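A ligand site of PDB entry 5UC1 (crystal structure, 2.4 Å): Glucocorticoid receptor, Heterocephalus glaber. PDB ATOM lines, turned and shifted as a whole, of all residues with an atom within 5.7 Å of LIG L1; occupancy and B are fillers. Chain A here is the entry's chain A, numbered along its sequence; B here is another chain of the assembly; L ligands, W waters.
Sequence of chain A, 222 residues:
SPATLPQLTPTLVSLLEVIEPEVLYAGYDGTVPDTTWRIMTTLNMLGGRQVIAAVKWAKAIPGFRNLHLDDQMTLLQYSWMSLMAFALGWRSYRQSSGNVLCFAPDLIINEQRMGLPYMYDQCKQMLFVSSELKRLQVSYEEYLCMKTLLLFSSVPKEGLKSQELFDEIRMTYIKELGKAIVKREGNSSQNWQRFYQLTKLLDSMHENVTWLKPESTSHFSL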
ATOM      1  N   MET A  40      25.624  -4.198 -18.685  1.00  0.00           N
ATOM      2  CA  MET A  40      25.859  -3.427 -19.895  1.00  0.00           C
ATOM      3  C   MET A  40      24.694  -3.540 -20.870  1.00  0.00           C
ATOM      4  O   MET A  40      24.299  -2.550 -21.490  1.00  0.00           O
ATOM      5  CB  MET A  40      27.150  -3.878 -20.577  1.00  0.00           C
ATOM      6  CG  MET A  40      28.422  -3.534 -19.827  1.00  0.00           C
ATOM      7  SD  MET A  40      29.866  -4.323 -20.624  1.00  0.00           S
ATOM      8  CE  MET A  40      29.777  -3.644 -22.274  1.00  0.00           C
ATOM      9  N   LEU A  43      21.868  -1.467 -19.454  1.00  0.00           N
ATOM     10  CA  LEU A  43      22.280  -0.074 -19.479  1.00  0.00           C
ATOM     11  C   LEU A  43      22.164   0.537 -20.858  1.00  0.00           C
ATOM     12  O   LEU A  43      21.828   1.721 -21.006  1.00  0.00           O
ATOM     13  CB  LEU A  43      23.706   0.013 -18.972  1.00  0.00           C
ATOM     14  CG  LEU A  43      24.432   1.345 -18.966  1.00  0.00           C
ATOM     15  CD1 LEU A  43      23.660   2.305 -18.077  1.00  0.00           C
ATOM     16  CD2 LEU A  43      25.803   1.115 -18.408  1.00  0.00           C
ATOM     17  N   ASN A  44      22.463  -0.249 -21.903  1.00  0.00           N
ATOM     18  CA  ASN A  44      22.356   0.277 -23.261  1.00  0.00           C
ATOM     19  C   ASN A  44      20.890   0.484 -23.644  1.00  0.00           C
ATOM     20  O   ASN A  44      20.587   1.398 -24.429  1.00  0.00           O
ATOM     21  CB  ASN A  44      23.059  -0.650 -24.254  1.00  0.00           C
ATOM     22  CG  ASN A  44      24.597  -0.607 -24.123  1.00  0.00           C
ATOM     23  OD1 ASN A  44      25.160   0.277 -23.454  1.00  0.00           O
ATOM     24  ND2 ASN A  44      25.278  -1.563 -24.761  1.00  0.00           N
ATOM     25  N   LEU A  46      18.545   1.346 -21.403  1.00  0.00           N
ATOM     26  CA  LEU A  46      18.264   2.548 -20.645  1.00  0.00           C
ATOM     27  C   LEU A  46      18.817   3.792 -21.341  1.00  0.00           C
ATOM     28  O   LEU A  46      18.134   4.826 -21.416  1.00  0.00           O
ATOM     29  CB  LEU A  46      18.866   2.404 -19.252  1.00  0.00           C
ATOM     30  CG  LEU A  46      18.683   3.623 -18.346  1.00  0.00           C
ATOM     31  CD1 LEU A  46      17.220   3.752 -17.991  1.00  0.00           C
ATOM     32  CD2 LEU A  46      19.494   3.495 -17.108  1.00  0.00           C
ATOM     33  N   GLY A  47      20.039   3.716 -21.841  1.00  0.00           N
ATOM     34  CA  GLY A  47      20.626   4.858 -22.524  1.00  0.00           C
ATOM     35  C   GLY A  47      19.838   5.261 -23.747  1.00  0.00           C
ATOM     36  O   GLY A  47      19.690   6.456 -24.020  1.00  0.00           O
ATOM     37  N   GLY A  48      19.321   4.277 -24.494  1.00  0.00           N
ATOM     38  CA  GLY A  48      18.531   4.606 -25.680  1.00  0.00           C
ATOM     39  C   GLY A  48      17.284   5.409 -25.333  1.00  0.00           C
ATOM     40  O   GLY A  48      16.903   6.322 -26.069  1.00  0.00           O
ATOM     41  N   GLN A  50      16.797   7.208 -22.406  1.00  0.00           N
ATOM     42  CA  GLN A  50      17.238   8.471 -21.839  1.00  0.00           C
ATOM     43  C   GLN A  50      17.576   9.495 -22.911  1.00  0.00           C
ATOM     44  O   GLN A  50      17.367  10.692 -22.710  1.00  0.00           O
ATOM     45  CB  GLN A  50      18.437   8.255 -20.929  1.00  0.00           C
ATOM     46  CG  GLN A  50      18.062   7.806 -19.529  1.00  0.00           C
ATOM     47  CD  GLN A  50      19.260   7.763 -18.621  1.00  0.00           C
ATOM     48  OE1 GLN A  50      20.356   8.166 -19.012  1.00  0.00           O
ATOM     49  NE2 GLN A  50      19.070   7.266 -17.417  1.00  0.00           N
ATOM     50  N   VAL A  51      18.116   9.055 -24.040  1.00  0.00           N
ATOM     51  CA  VAL A  51      18.361   9.993 -25.126  1.00  0.00           C
ATOM     52  C   VAL A  51      17.040  10.568 -25.614  1.00  0.00           C
ATOM     53  O   VAL A  51      16.937  11.774 -25.899  1.00  0.00           O
ATOM     54  CB  VAL A  51      19.126   9.318 -26.290  1.00  0.00           C
ATOM     55  CG1 VAL A  51      19.398  10.334 -27.362  1.00  0.00           C
ATOM     56  CG2 VAL A  51      20.412   8.746 -25.805  1.00  0.00           C
ATOM     57  N   TRP A  80      24.289  15.939 -25.954  1.00  0.00           N
ATOM     58  CA  TRP A  80      23.321  14.966 -25.444  1.00  0.00           C
ATOM     59  C   TRP A  80      23.912  14.025 -24.399  1.00  0.00           C
ATOM     60  O   TRP A  80      23.262  13.733 -23.392  1.00  0.00           O
ATOM     61  CB  TRP A  80      22.695  14.198 -26.601  1.00  0.00           C
ATOM     62  CG  TRP A  80      23.576  13.286 -27.437  1.00  0.00           C
ATOM     63  CD1 TRP A  80      24.202  13.596 -28.612  1.00  0.00           C
ATOM     64  CD2 TRP A  80      23.836  11.900 -27.207  1.00  0.00           C
ATOM     65  NE1 TRP A  80      24.853  12.491 -29.108  1.00  0.00           N
ATOM     66  CE2 TRP A  80      24.643  11.437 -28.263  1.00  0.00           C
ATOM     67  CE3 TRP A  80      23.474  10.997 -26.194  1.00  0.00           C
ATOM     68  CZ2 TRP A  80      25.117  10.108 -28.339  1.00  0.00           C
ATOM     69  CZ3 TRP A  80      23.939   9.664 -26.273  1.00  0.00           C
ATOM     70  CH2 TRP A  80      24.755   9.240 -27.340  1.00  0.00           C
ATOM     71  N   MET A  81      25.134  13.542 -24.604  1.00  0.00           N
ATOM     72  CA  MET A  81      25.682  12.614 -23.615  1.00  0.00           C
ATOM     73  C   MET A  81      26.197  13.361 -22.390  1.00  0.00           C
ATOM     74  O   MET A  81      26.154  12.828 -21.274  1.00  0.00           O
ATOM     75  CB  MET A  81      26.784  11.738 -24.219  1.00  0.00           C
ATOM     76  CG  MET A  81      26.991  10.429 -23.446  1.00  0.00           C
ATOM     77  SD  MET A  81      28.363   9.393 -23.966  1.00  0.00           S
ATOM     78  CE  MET A  81      27.958   9.084 -25.678  1.00  0.00           C
ATOM     79  N   MET A  84      23.216  13.671 -20.101  1.00  0.00           N
ATOM     80  CA  MET A  84      22.886  12.420 -19.421  1.00  0.00           C
ATOM     81  C   MET A  84      23.885  12.094 -18.316  1.00  0.00           C
ATOM     82  O   MET A  84      23.511  11.615 -17.239  1.00  0.00           O
ATOM     83  CB  MET A  84      22.824  11.287 -20.442  1.00  0.00           C
ATOM     84  CG  MET A  84      21.615  11.344 -21.367  1.00  0.00           C
ATOM     85  SD  MET A  84      21.732  10.235 -22.776  1.00  0.00           S
ATOM     86  CE  MET A  84      22.088   8.667 -21.967  1.00  0.00           C
ATOM     87  N   ALA A  85      25.170  12.329 -18.589  1.00  0.00           N
ATOM     88  CA  ALA A  85      26.179  12.210 -17.559  1.00  0.00           C
ATOM     89  C   ALA A  85      25.957  13.204 -16.428  1.00  0.00           C
ATOM     90  O   ALA A  85      26.170  12.876 -15.256  1.00  0.00           O
ATOM     91  CB  ALA A  85      27.559  12.414 -18.179  1.00  0.00           C
ATOM     92  N   LEU A  88      23.120  12.035 -14.446  1.00  0.00           N
ATOM     93  CA  LEU A  88      23.584  10.864 -13.715  1.00  0.00           C
ATOM     94  C   LEU A  88      24.357  11.263 -12.471  1.00  0.00           C
ATOM     95  O   LEU A  88      24.084  10.774 -11.365  1.00  0.00           O
ATOM     96  CB  LEU A  88      24.463   9.989 -14.623  1.00  0.00           C
ATOM     97  CG  LEU A  88      25.200   8.816 -13.982  1.00  0.00           C
ATOM     98  CD1 LEU A  88      24.221   7.811 -13.376  1.00  0.00           C
ATOM     99  CD2 LEU A  88      26.139   8.140 -14.987  1.00  0.00           C
ATOM    100  N   ARG A  91      21.787  12.446  -9.770  1.00  0.00           N
ATOM    101  CA  ARG A  91      21.126  11.307  -9.140  1.00  0.00           C
ATOM    102  C   ARG A  91      22.058  10.556  -8.203  1.00  0.00           C
ATOM    103  O   ARG A  91      21.663  10.136  -7.116  1.00  0.00           O
ATOM    104  CB  ARG A  91      20.574  10.350 -10.191  1.00  0.00           C
ATOM    105  CG  ARG A  91      19.461  10.882 -11.055  1.00  0.00           C
ATOM    106  CD  ARG A  91      18.788   9.743 -11.818  1.00  0.00           C
ATOM    107  NE  ARG A  91      19.669   9.057 -12.754  1.00  0.00           N
ATOM    108  CZ  ARG A  91      19.954   9.468 -13.999  1.00  0.00           C
ATOM    109  NH1 ARG A  91      19.428  10.583 -14.476  1.00  0.00           N
ATOM    110  NH2 ARG A  91      20.755   8.759 -14.769  1.00  0.00           N
ATOM    111  N   CYS A 102      24.319   5.945  -9.872  1.00  0.00           N
ATOM    112  CA  CYS A 102      22.902   5.653  -9.822  1.00  0.00           C
ATOM    113  C   CYS A 102      22.307   5.830 -11.218  1.00  0.00           C
ATOM    114  O   CYS A 102      21.715   6.860 -11.543  1.00  0.00           O
ATOM    115  CB  CYS A 102      22.233   6.565  -8.776  1.00  0.00           C
ATOM    116  SG  CYS A 102      20.470   6.435  -8.714  1.00  0.00           S
ATOM    117  N   PHE A 103      22.485   4.814 -12.063  1.00  0.00           N
ATOM    118  CA  PHE A 103      21.957   4.900 -13.424  1.00  0.00           C
ATOM    119  C   PHE A 103      20.445   4.974 -13.412  1.00  0.00           C
ATOM    120  O   PHE A 103      19.849   5.676 -14.237  1.00  0.00           O
ATOM    121  CB  PHE A 103      22.406   3.717 -14.269  1.00  0.00           C
ATOM    122  CG  PHE A 103      23.880   3.714 -14.570  1.00  0.00           C
ATOM    123  CD1 PHE A 103      24.443   4.712 -15.341  1.00  0.00           C
ATOM    124  CD2 PHE A 103      24.700   2.726 -14.067  1.00  0.00           C
ATOM    125  CE1 PHE A 103      25.790   4.725 -15.612  1.00  0.00           C
ATOM    126  CE2 PHE A 103      26.076   2.737 -14.347  1.00  0.00           C
ATOM    127  CZ  PHE A 103      26.610   3.736 -15.109  1.00  0.00           C
ATOM    128  N   ALA A 104      19.829   4.269 -12.483  1.00  0.00           N
ATOM    129  CA  ALA A 104      18.383   4.200 -12.339  1.00  0.00           C
ATOM    130  C   ALA A 104      18.105   3.728 -10.919  1.00  0.00           C
ATOM    131  O   ALA A 104      19.019   3.243 -10.235  1.00  0.00           O
ATOM    132  CB  ALA A 104      17.761   3.249 -13.370  1.00  0.00           C
ATOM    133  N   MET A 119      33.990  -3.376 -15.376  1.00  0.00           N
ATOM    134  CA  MET A 119      32.967  -2.413 -14.957  1.00  0.00           C
ATOM    135  C   MET A 119      33.574  -1.107 -14.475  1.00  0.00           C
ATOM    136  O   MET A 119      33.207  -0.029 -14.947  1.00  0.00           O
ATOM    137  CB  MET A 119      32.079  -3.030 -13.876  1.00  0.00           C
ATOM    138  CG  MET A 119      30.774  -2.299 -13.649  1.00  0.00           C
ATOM    139  SD  MET A 119      29.825  -2.062 -15.152  1.00  0.00           S
ATOM    140  CE  MET A 119      29.480  -3.762 -15.595  1.00  0.00           C
ATOM    141  N   GLN A 122      35.018   0.975 -17.359  1.00  0.00           N
ATOM    142  CA  GLN A 122      33.967   1.655 -18.118  1.00  0.00           C
ATOM    143  C   GLN A 122      33.296   2.775 -17.322  1.00  0.00           C
ATOM    144  O   GLN A 122      32.700   3.654 -17.925  1.00  0.00           O
ATOM    145  CB  GLN A 122      32.889   0.651 -18.539  1.00  0.00           C
ATOM    146  CG  GLN A 122      33.276  -0.303 -19.628  1.00  0.00           C
ATOM    147  CD  GLN A 122      32.191  -1.334 -19.879  1.00  0.00           C
ATOM    148  OE1 GLN A 122      31.238  -1.088 -20.641  1.00  0.00           O
ATOM    149  NE2 GLN A 122      32.307  -2.486 -19.221  1.00  0.00           N
ATOM    150  N   CYS A 123      33.369   2.743 -15.989  1.00  0.00           N
ATOM    151  CA  CYS A 123      32.639   3.673 -15.137  1.00  0.00           C
ATOM    152  C   CYS A 123      33.482   4.830 -14.615  1.00  0.00           C
ATOM    153  O   CYS A 123      32.931   5.905 -14.359  1.00  0.00           O
ATOM    154  CB  CYS A 123      32.074   2.922 -13.926  1.00  0.00           C
ATOM    155  SG  CYS A 123      30.589   1.904 -14.259  1.00  0.00           S
ATOM    156  N   MET A 126      32.944   8.777 -15.006  1.00  0.00           N
ATOM    157  CA  MET A 126      31.676   9.360 -14.571  1.00  0.00           C
ATOM    158  C   MET A 126      31.635   9.665 -13.072  1.00  0.00           C
ATOM    159  O   MET A 126      30.787  10.450 -12.635  1.00  0.00           O
ATOM    160  CB  MET A 126      30.531   8.429 -14.944  1.00  0.00           C
ATOM    161  CG  MET A 126      30.268   8.371 -16.433  1.00  0.00           C
ATOM    162  SD  MET A 126      29.091   7.089 -16.914  1.00  0.00           S
ATOM    163  CE  MET A 126      30.148   5.633 -17.133  1.00  0.00           C
ATOM    164  N   TRP B  37      25.066   8.607 -32.537  1.00  0.00           N
ATOM    165  CA  TRP B  37      23.968   7.769 -32.078  1.00  0.00           C
ATOM    166  C   TRP B  37      23.825   6.518 -32.957  1.00  0.00           C
ATOM    167  O   TRP B  37      23.570   5.420 -32.446  1.00  0.00           O
ATOM    168  CB  TRP B  37      22.682   8.586 -32.066  1.00  0.00           C
ATOM    169  CG  TRP B  37      21.525   7.863 -31.452  1.00  0.00           C
ATOM    170  CD1 TRP B  37      21.167   7.826 -30.132  1.00  0.00           C
ATOM    171  CD2 TRP B  37      20.578   7.052 -32.141  1.00  0.00           C
ATOM    172  NE1 TRP B  37      20.064   7.040 -29.958  1.00  0.00           N
ATOM    173  CE2 TRP B  37      19.679   6.554 -31.178  1.00  0.00           C
ATOM    174  CE3 TRP B  37      20.407   6.714 -33.484  1.00  0.00           C
ATOM    175  CZ2 TRP B  37      18.617   5.719 -31.520  1.00  0.00           C
ATOM    176  CZ3 TRP B  37      19.362   5.863 -33.822  1.00  0.00           C
ATOM    177  CH2 TRP B  37      18.488   5.378 -32.848  1.00  0.00           C
ATOM    178  N   MET B  40      26.922   4.076 -32.202  1.00  0.00           N
ATOM    179  CA  MET B  40      26.866   3.399 -30.905  1.00  0.00           C
ATOM    180  C   MET B  40      25.728   2.397 -30.852  1.00  0.00           C
ATOM    181  O   MET B  40      25.849   1.357 -30.197  1.00  0.00           O
ATOM    182  CB  MET B  40      26.687   4.423 -29.798  1.00  0.00           C
ATOM    183  CG  MET B  40      27.874   5.306 -29.531  1.00  0.00           C
ATOM    184  SD  MET B  40      27.388   6.646 -28.374  1.00  0.00           S
ATOM    185  CE  MET B  40      26.961   5.733 -26.894  1.00  0.00           C
ATOM    186  N   THR B  41      24.600   2.713 -31.473  1.00  0.00           N
ATOM    187  CA  THR B  41      23.456   1.803 -31.401  1.00  0.00           C
ATOM    188  C   THR B  41      23.728   0.541 -32.207  1.00  0.00           C
ATOM    189  O   THR B  41      23.378  -0.571 -31.797  1.00  0.00           O
ATOM    190  CB  THR B  41      22.179   2.499 -31.882  1.00  0.00           C
ATOM    191  OG1 THR B  41      21.813   3.570 -30.989  1.00  0.00           O
ATOM    192  CG2 THR B  41      21.019   1.517 -31.947  1.00  0.00           C
ATOM    193  N   ASN B  44      26.556  -1.533 -30.407  1.00  0.00           N
ATOM    194  CA  ASN B  44      26.101  -2.327 -29.269  1.00  0.00           C
ATOM    195  C   ASN B  44      25.421  -3.608 -29.720  1.00  0.00           C
ATOM    196  O   ASN B  44      25.582  -4.660 -29.091  1.00  0.00           O
ATOM    197  CB  ASN B  44      25.166  -1.499 -28.372  1.00  0.00           C
ATOM    198  CG  ASN B  44      25.899  -0.347 -27.630  1.00  0.00           C
ATOM    199  OD1 ASN B  44      27.136  -0.306 -27.544  1.00  0.00           O
ATOM    200  ND2 ASN B  44      25.107   0.588 -27.075  1.00  0.00           N
ATOM    201  N   GLN B 122      35.422   7.818 -26.412  1.00  0.00           N
ATOM    202  CA  GLN B 122      34.979   6.430 -26.258  1.00  0.00           C
ATOM    203  C   GLN B 122      35.915   5.416 -26.927  1.00  0.00           C
ATOM    204  O   GLN B 122      35.930   4.251 -26.534  1.00  0.00           O
ATOM    205  CB  GLN B 122      33.588   6.257 -26.860  1.00  0.00           C
ATOM    206  CG  GLN B 122      32.434   6.646 -26.002  1.00  0.00           C
ATOM    207  CD  GLN B 122      31.125   6.316 -26.677  1.00  0.00           C
ATOM    208  OE1 GLN B 122      30.580   5.216 -26.502  1.00  0.00           O
ATOM    209  NE2 GLN B 122      30.632   7.233 -27.492  1.00  0.00           N
HETATM  210  O1  LIG L   1      22.039   7.506 -16.573  1.00  0.00           O
HETATM  211  C1  LIG L   1      22.679   7.183 -17.563  1.00  0.00           C
HETATM  212  C2  LIG L   1      22.531   5.781 -18.158  1.00  0.00           C
HETATM  213  C3  LIG L   1      23.657   8.098 -18.175  1.00  0.00           C
HETATM  214  C4  LIG L   1      24.462   7.744 -19.213  1.00  0.00           C
HETATM  215  C5  LIG L   1      25.487   8.710 -19.709  1.00  0.00           C
HETATM  216  C6  LIG L   1      24.415   6.399 -19.834  1.00  0.00           C
HETATM  217  C7  LIG L   1      23.159   5.592 -19.548  1.00  0.00           C
HETATM  218  C8  LIG L   1      25.422   5.932 -20.613  1.00  0.00           C
HETATM  219  C9  LIG L   1      25.323   4.570 -21.320  1.00  0.00           C
HETATM  220  C10 LIG L   1      24.665   4.663 -22.691  1.00  0.00           C
HETATM  221  C11 LIG L   1      24.512   3.501 -23.447  1.00  0.00           C
HETATM  222  C12 LIG L   1      23.919   3.515 -24.706  1.00  0.00           C
HETATM  223  C13 LIG L   1      23.442   4.725 -25.274  1.00  0.00           C
HETATM  224  N1  LIG L   1      22.835   4.767 -26.530  1.00  0.00           N
HETATM  225  C14 LIG L   1      22.453   6.042 -27.119  1.00  0.00           C
HETATM  226  C15 LIG L   1      22.042   3.621 -26.982  1.00  0.00           C
HETATM  227  C16 LIG L   1      23.575   5.888 -24.496  1.00  0.00           C
HETATM  228  C17 LIG L   1      24.178   5.859 -23.245  1.00  0.00           C
HETATM  229  C18 LIG L   1      26.690   3.821 -21.353  1.00  0.00           C
HETATM  230  C19 LIG L   1      27.912   4.673 -21.696  1.00  0.00           C
HETATM  231  C20 LIG L   1      27.880   5.193 -23.143  1.00  0.00           C
HETATM  232  C21 LIG L   1      29.331   4.033 -21.460  1.00  0.00           C
HETATM  233  C22 LIG L   1      29.357   3.199 -20.259  1.00  0.00           C
HETATM  234  C23 LIG L   1      29.357   2.529 -19.256  1.00  0.00           C
HETATM  235  C24 LIG L   1      29.357   1.737 -18.044  1.00  0.00           C
HETATM  236  O2  LIG L   1      29.715   3.254 -22.609  1.00  0.00           O
HETATM  237  C25 LIG L   1      30.260   5.262 -21.212  1.00  0.00           C
HETATM  238  C26 LIG L   1      29.338   6.453 -20.764  1.00  0.00           C
HETATM  239  C27 LIG L   1      27.928   5.823 -20.669  1.00  0.00           C
HETATM  240  C28 LIG L   1      26.703   6.739 -20.814  1.00  0.00           C
HETATM  241  C29 LIG L   1      26.801   7.940 -19.877  1.00  0.00           C
HETATM  242  O1  LG2 L   2      34.683  -5.348 -32.697  1.00  0.00           O
HETATM  243  C1  LG2 L   2      34.221  -5.026 -31.619  1.00  0.00           C
HETATM  244  C2  LG2 L   2      32.825  -4.394 -31.577  1.00  0.00           C
HETATM  245  C3  LG2 L   2      34.985  -5.112 -30.373  1.00  0.00           C
HETATM  246  C4  LG2 L   2      34.525  -4.621 -29.182  1.00  0.00           C
HETATM  247  C5  LG2 L   2      35.389  -4.655 -27.953  1.00  0.00           C
HETATM  248  C6  LG2 L   2      33.216  -3.950 -29.049  1.00  0.00           C
HETATM  249  C7  LG2 L   2      32.229  -4.260 -30.169  1.00  0.00           C
HETATM  250  C8  LG2 L   2      32.902  -3.171 -27.986  1.00  0.00           C
HETATM  251  C9  LG2 L   2      31.513  -2.523 -27.864  1.00  0.00           C
HETATM  252  C10 LG2 L   2      30.488  -3.404 -27.177  1.00  0.00           C
HETATM  253  C11 LG2 L   2      29.164  -2.967 -27.046  1.00  0.00           C
HETATM  254  C12 LG2 L   2      28.195  -3.729 -26.410  1.00  0.00           C
HETATM  255  C13 LG2 L   2      28.502  -5.007 -25.866  1.00  0.00           C
HETATM  256  N1  LG2 L   2      27.552  -5.808 -25.229  1.00  0.00           N
HETATM  257  C14 LG2 L   2      28.008  -6.931 -24.423  1.00  0.00           C
HETATM  258  C15 LG2 L   2      26.204  -5.899 -25.777  1.00  0.00           C
HETATM  259  C16 LG2 L   2      29.835  -5.429 -26.011  1.00  0.00           C
HETATM  260  C17 LG2 L   2      30.797  -4.641 -26.631  1.00  0.00           C
HETATM  261  C18 LG2 L   2      31.558  -1.095 -27.253  1.00  0.00           C
HETATM  262  C19 LG2 L   2      32.454  -0.940 -26.012  1.00  0.00           C
HETATM  263  C20 LG2 L   2      31.900  -1.704 -24.785  1.00  0.00           C
HETATM  264  C21 LG2 L   2      32.739   0.543 -25.565  1.00  0.00           C
HETATM  265  C22 LG2 L   2      32.893   1.391 -26.727  1.00  0.00           C
HETATM  266  C23 LG2 L   2      33.057   2.020 -27.737  1.00  0.00           C
HETATM  267  C24 LG2 L   2      33.311   2.749 -28.971  1.00  0.00           C
HETATM  268  O2  LG2 L   2      31.647   1.010 -24.748  1.00  0.00           O
HETATM  269  C25 LG2 L   2      34.099   0.414 -24.808  1.00  0.00           C
HETATM  270  C26 LG2 L   2      34.816  -0.859 -25.351  1.00  0.00           C
HETATM  271  C27 LG2 L   2      33.857  -1.388 -26.446  1.00  0.00           C
HETATM  272  C28 LG2 L   2      33.908  -2.867 -26.879  1.00  0.00           C
HETATM  273  C29 LG2 L   2      35.339  -3.300 -27.254  1.00  0.00           C
HETATM  274  O   HOH W   1      21.018  10.337 -17.132  1.00  0.00           O
HETATM  275  O   HOH W   2      27.578   0.611 -23.126  1.00  0.00           O
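Merely in contact with LIG L1: Asn 44 of chain A (3.3 Å), Phe 103 (3.6 Å), Leu 43 (3.6 Å), Val 51 (3.6 Å), Met 84 (3.6 Å), Gly 47 (3.7 Å), Gln 122 of chain A (3.7 Å), Trp 37 of chain B (3.7 Å), Gly 48 (3.7 Å), Ala 85 (3.8 Å), Met 126 (3.8 Å), Leu 88 (3.9 Å), Met 40 of chain B (3.9 Å), Leu 46 (3.9 Å), Trp 80 (3.9 Å), Asn 44 of chain B (3.9 Å) and Cys 123 (3.98 Å).
Hydrophobic or aromatic side chains that line LIG L1: Leu 43, Leu 46, Val 51, Trp 80, Met 84, Leu 88, Phe 103, Met 126, Trp 37 of chain B and Met 40 of chain B.
Of the 26 residues printed, 19 come within 4 Å of LIG L1.
Water W2 lies within hydrogen-bond range of OD1 of Asn 44 of chain A (2.5 Å) and O2 of LIG L1 (3.4 Å).
OE1 of Gln 50 lies close to O1 of LIG L1 (3.0 Å).
NH2 of Arg 91 sits at hydrogen-bond distance from O1 of LIG L1, 2.5 Å away.
The side-chain amide nitrogen of Asn 44 of chain A sits close to the side-chain amide nitrogen of Asn 44 of chain B (3.2 Å).
The guanidinium group (NH2) of Arg 91 is in hydrogen-bond range of the backbone carbonyl oxygen (O) of Phe 103, 3.3 Å away.
The side-chain sulfur of Cys 123 lies close to the backbone carbonyl oxygen of Met 119 (3.3 Å).
The guanidinium group (NH2) of Arg 91 sits close to the side-chain amide nitrogen (NE2) of Gln 50, at 3.5 Å.
The backbone carbonyl oxygen (O) of Met 40 of chain B sits close to the side-chain amide nitrogen (ND2) of Asn 44 of chain B, at 3.3 Å.
The side-chain hydroxyl (OG1) of Thr 41 of chain B is in hydrogen-bond range of the backbone carbonyl oxygen (O) of Trp 37 of chain B.
SD of Met 40 of chain B lies within hydrogen-bond range of NE2 of Gln 122 of chain B, at 3.4 Å.
The side-chain amide nitrogen (NE2) of Gln 122 of chain A sits at hydrogen-bond distance from the side-chain sulfur (SD) of Met 40 of chain A (3.4 Å).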
